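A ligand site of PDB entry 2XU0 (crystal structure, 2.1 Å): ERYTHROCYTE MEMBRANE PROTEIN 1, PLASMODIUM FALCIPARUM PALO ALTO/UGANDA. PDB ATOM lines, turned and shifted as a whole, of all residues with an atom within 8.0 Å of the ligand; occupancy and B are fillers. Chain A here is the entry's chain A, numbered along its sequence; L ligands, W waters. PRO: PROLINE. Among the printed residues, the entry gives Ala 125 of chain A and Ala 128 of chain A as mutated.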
ATOM      1  N   GLU A 122      -8.548 -12.593  12.376  1.00  0.00           N
ATOM      2  CA  GLU A 122      -7.747 -13.727  12.844  1.00  0.00           C
ATOM      3  C   GLU A 122      -6.756 -14.118  11.764  1.00  0.00           C
ATOM      4  O   GLU A 122      -6.995 -13.853  10.591  1.00  0.00           O
ATOM      5  CB  GLU A 122      -8.650 -14.918  13.184  1.00  0.00           C
ATOM      6  CG  GLU A 122      -9.577 -14.756  14.397  1.00  0.00           C
ATOM      7  CD  GLU A 122      -8.984 -14.282  15.715  1.00  0.00           C
ATOM      8  OE1 GLU A 122      -7.786 -14.541  16.001  1.00  0.00           O
ATOM      9  OE2 GLU A 122      -9.749 -13.654  16.488  1.00  0.00           O
ATOM     10  N   ASN A 123      -5.646 -14.736  12.161  1.00  0.00           N
ATOM     11  CA  ASN A 123      -4.626 -15.196  11.200  1.00  0.00           C
ATOM     12  C   ASN A 123      -5.185 -16.298  10.315  1.00  0.00           C
ATOM     13  O   ASN A 123      -4.758 -16.390   9.172  1.00  0.00           O
ATOM     14  CB  ASN A 123      -3.375 -15.704  11.933  1.00  0.00           C
ATOM     15  CG  ASN A 123      -2.547 -14.637  12.601  1.00  0.00           C
ATOM     16  OD1 ASN A 123      -2.100 -14.799  13.737  1.00  0.00           O
ATOM     17  ND2 ASN A 123      -2.306 -13.533  11.919  1.00  0.00           N
ATOM     18  N   ASN A 124      -6.171 -17.084  10.796  1.00  0.00           N
ATOM     19  CA  ASN A 124      -6.769 -18.189  10.021  1.00  0.00           C
ATOM     20  C   ASN A 124      -7.850 -17.760   9.003  1.00  0.00           C
ATOM     21  O   ASN A 124      -8.555 -18.618   8.443  1.00  0.00           O
ATOM     22  CB  ASN A 124      -7.277 -19.320  10.944  1.00  0.00           C
ATOM     23  CG  ASN A 124      -8.361 -18.914  11.930  1.00  0.00           C
ATOM     24  OD1 ASN A 124      -9.003 -17.867  11.823  1.00  0.00           O
ATOM     25  ND2 ASN A 124      -8.593 -19.747  12.918  1.00  0.00           N
ATOM     26  N   ALA A 125      -7.983 -16.442   8.790  1.00  0.00           N
ATOM     27  CA  ALA A 125      -8.955 -15.913   7.837  1.00  0.00           C
ATOM     28  C   ALA A 125      -8.376 -14.784   6.989  1.00  0.00           C
ATOM     29  O   ALA A 125      -7.734 -13.864   7.517  1.00  0.00           O
ATOM     30  CB  ALA A 125     -10.222 -15.454   8.556  1.00  0.00           C
ATOM     31  N   ASN A 126      -8.594 -14.871   5.669  1.00  0.00           N
ATOM     32  CA  ASN A 126      -8.169 -13.812   4.728  1.00  0.00           C
ATOM     33  C   ASN A 126      -9.084 -12.586   4.863  1.00  0.00           C
ATOM     34  O   ASN A 126      -8.583 -11.465   4.816  1.00  0.00           O
ATOM     35  CB  ASN A 126      -8.111 -14.308   3.291  1.00  0.00           C
ATOM     36  CG  ASN A 126      -7.020 -15.310   3.060  1.00  0.00           C
ATOM     37  OD1 ASN A 126      -5.824 -14.993   3.186  1.00  0.00           O
ATOM     38  ND2 ASN A 126      -7.405 -16.547   2.780  1.00  0.00           N
ATOM     39  N   GLY A 127     -10.375 -12.818   5.092  1.00  0.00           N
ATOM     40  CA  GLY A 127     -11.355 -11.738   5.290  1.00  0.00           C
ATOM     41  C   GLY A 127     -10.997 -10.892   6.491  1.00  0.00           C
ATOM     42  O   GLY A 127     -10.734 -11.441   7.571  1.00  0.00           O
ATOM     43  N   ALA A 128     -10.939  -9.561   6.307  1.00  0.00           N
ATOM     44  CA  ALA A 128     -10.495  -8.673   7.396  1.00  0.00           C
ATOM     45  C   ALA A 128     -11.048  -7.271   7.318  1.00  0.00           C
ATOM     46  O   ALA A 128     -11.245  -6.729   6.236  1.00  0.00           O
ATOM     47  CB  ALA A 128      -8.969  -8.619   7.416  1.00  0.00           C
ATOM     48  N   TYR A 392      -9.229  -6.846  -1.394  1.00  0.00           N
ATOM     49  CA  TYR A 392      -9.754  -8.231  -1.382  1.00  0.00           C
ATOM     50  C   TYR A 392     -10.118  -8.673   0.040  1.00  0.00           C
ATOM     51  O   TYR A 392     -11.130  -9.349   0.221  1.00  0.00           O
ATOM     52  CB  TYR A 392      -8.746  -9.238  -1.980  1.00  0.00           C
ATOM     53  CG  TYR A 392      -8.562  -9.172  -3.475  1.00  0.00           C
ATOM     54  CD1 TYR A 392      -9.658  -9.111  -4.339  1.00  0.00           C
ATOM     55  CD2 TYR A 392      -7.295  -9.363  -4.046  1.00  0.00           C
ATOM     56  CE1 TYR A 392      -9.499  -9.180  -5.724  1.00  0.00           C
ATOM     57  CE2 TYR A 392      -7.122  -9.389  -5.431  1.00  0.00           C
ATOM     58  CZ  TYR A 392      -8.225  -9.291  -6.260  1.00  0.00           C
ATOM     59  OH  TYR A 392      -8.039  -9.266  -7.613  1.00  0.00           O
ATOM     60  N   LYS A 393      -9.332  -8.231   1.044  1.00  0.00           N
ATOM     61  CA  LYS A 393      -9.569  -8.593   2.449  1.00  0.00           C
ATOM     62  C   LYS A 393     -10.891  -8.055   2.940  1.00  0.00           C
ATOM     63  O   LYS A 393     -11.574  -8.737   3.690  1.00  0.00           O
ATOM     64  CB  LYS A 393      -8.456  -8.085   3.345  1.00  0.00           C
ATOM     65  CG  LYS A 393      -7.140  -8.866   3.220  1.00  0.00           C
ATOM     66  CD  LYS A 393      -6.171  -8.254   4.149  1.00  0.00           C
ATOM     67  CE  LYS A 393      -5.206  -9.278   4.700  1.00  0.00           C
ATOM     68  NZ  LYS A 393      -3.854  -9.085   4.101  1.00  0.00           N
ATOM     69  N   ASN A 395     -13.407  -7.126   0.925  1.00  0.00           N
ATOM     70  CA  ASN A 395     -14.339  -7.738   0.004  1.00  0.00           C
ATOM     71  C   ASN A 395     -14.836  -9.035   0.641  1.00  0.00           C
ATOM     72  O   ASN A 395     -16.039  -9.294   0.669  1.00  0.00           O
ATOM     73  CB  ASN A 395     -13.600  -8.023  -1.311  1.00  0.00           C
ATOM     74  CG  ASN A 395     -14.429  -8.535  -2.444  1.00  0.00           C
ATOM     75  OD1 ASN A 395     -15.252  -9.450  -2.317  1.00  0.00           O
ATOM     76  ND2 ASN A 395     -14.171  -7.980  -3.598  1.00  0.00           N
ATOM     77  N   LEU A 396     -13.906  -9.820   1.181  1.00  0.00           N
ATOM     78  CA  LEU A 396     -14.222 -11.071   1.873  1.00  0.00           C
ATOM     79  C   LEU A 396     -14.981 -10.796   3.178  1.00  0.00           C
ATOM     80  O   LEU A 396     -15.966 -11.482   3.468  1.00  0.00           O
ATOM     81  CB  LEU A 396     -12.937 -11.876   2.165  1.00  0.00           C
ATOM     82  CG  LEU A 396     -12.262 -12.523   0.975  1.00  0.00           C
ATOM     83  CD1 LEU A 396     -10.838 -12.914   1.308  1.00  0.00           C
ATOM     84  CD2 LEU A 396     -13.006 -13.758   0.535  1.00  0.00           C
ATOM     85  N   LYS A 397     -14.536  -9.813   3.963  1.00  0.00           N
ATOM     86  CA  LYS A 397     -15.175  -9.460   5.220  1.00  0.00           C
ATOM     87  C   LYS A 397     -16.627  -9.053   4.996  1.00  0.00           C
ATOM     88  O   LYS A 397     -17.461  -9.365   5.836  1.00  0.00           O
ATOM     89  CB  LYS A 397     -14.409  -8.343   5.964  1.00  0.00           C
ATOM     90  CG  LYS A 397     -14.892  -8.113   7.435  1.00  0.00           C
ATOM     91  CD  LYS A 397     -14.644  -9.354   8.263  1.00  0.00           C
ATOM     92  CE  LYS A 397     -14.830  -9.185   9.747  1.00  0.00           C
ATOM     93  NZ  LYS A 397     -14.515 -10.467  10.436  1.00  0.00           N
ATOM     94  N   SER A 399     -18.701 -10.065   2.499  1.00  0.00           N
ATOM     95  CA  SER A 399     -19.422 -11.304   2.259  1.00  0.00           C
ATOM     96  C   SER A 399     -19.730 -12.038   3.599  1.00  0.00           C
ATOM     97  O   SER A 399     -20.855 -12.431   3.843  1.00  0.00           O
ATOM     98  CB  SER A 399     -18.603 -12.185   1.321  1.00  0.00           C
ATOM     99  OG  SER A 399     -19.255 -13.433   1.101  1.00  0.00           O
ATOM    100  N   MET A 400     -18.726 -12.137   4.471  1.00  0.00           N
ATOM    101  CA  MET A 400     -18.815 -12.754   5.786  1.00  0.00           C
ATOM    102  C   MET A 400     -19.836 -12.062   6.689  1.00  0.00           C
ATOM    103  O   MET A 400     -20.594 -12.761   7.350  1.00  0.00           O
ATOM    104  CB  MET A 400     -17.437 -12.782   6.470  1.00  0.00           C
ATOM    105  CG  MET A 400     -16.482 -13.781   5.822  1.00  0.00           C
ATOM    106  SD  MET A 400     -14.768 -13.458   6.291  1.00  0.00           S
ATOM    107  CE  MET A 400     -14.763 -14.091   7.966  1.00  0.00           C
ATOM    108  N   GLN A 403     -23.249 -12.928   5.276  1.00  0.00           N
ATOM    109  CA  GLN A 403     -23.497 -14.358   5.581  1.00  0.00           C
ATOM    110  C   GLN A 403     -23.841 -14.581   7.046  1.00  0.00           C
ATOM    111  O   GLN A 403     -24.698 -15.416   7.363  1.00  0.00           O
ATOM    112  CB  GLN A 403     -22.292 -15.259   5.192  1.00  0.00           C
ATOM    113  CG  GLN A 403     -22.068 -15.436   3.683  1.00  0.00           C
ATOM    114  CD  GLN A 403     -23.318 -15.820   2.924  1.00  0.00           C
ATOM    115  OE1 GLN A 403     -23.761 -15.097   2.026  1.00  0.00           O
ATOM    116  NE2 GLN A 403     -23.933 -16.935   3.285  1.00  0.00           N
HETATM  117  N   PRO L   1     -13.712 -17.182   5.225  1.00  0.00           N
HETATM  118  CA  PRO L   1     -12.519 -17.282   4.349  1.00  0.00           C
HETATM  119  C   PRO L   1     -11.449 -16.258   4.745  1.00  0.00           C
HETATM  120  O   PRO L   1     -11.820 -15.178   5.285  1.00  0.00           O
HETATM  121  CB  PRO L   1     -13.087 -17.000   2.938  1.00  0.00           C
HETATM  122  CG  PRO L   1     -14.406 -16.279   3.170  1.00  0.00           C
HETATM  123  CD  PRO L   1     -14.924 -16.802   4.481  1.00  0.00           C
HETATM  124  OXT PRO L   1     -10.252 -16.519   4.463  1.00  0.00           O
HETATM  125  O   HOH W   1     -13.480 -18.294   8.130  1.00  0.00           O
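N of Asn 126 sits at hydrogen-bond distance from OXT of the ligand.
ND2 of Asn 126 sits close to OXT of the ligand (3.3 Å).
O of the ligand is in hydrogen-bond range of N of Gly 127 (2.8 Å).
The side-chain sulfur of Met 400 lies close to an oxygen (O) of the ligand.
C of Ala 125 touches OXT of the ligand (3.6 Å).
Leu 396 touches the ligand (CD2 to CG, 3.9 Å).
Of the 15 residues printed, 5 come within 4 Å of the ligand.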
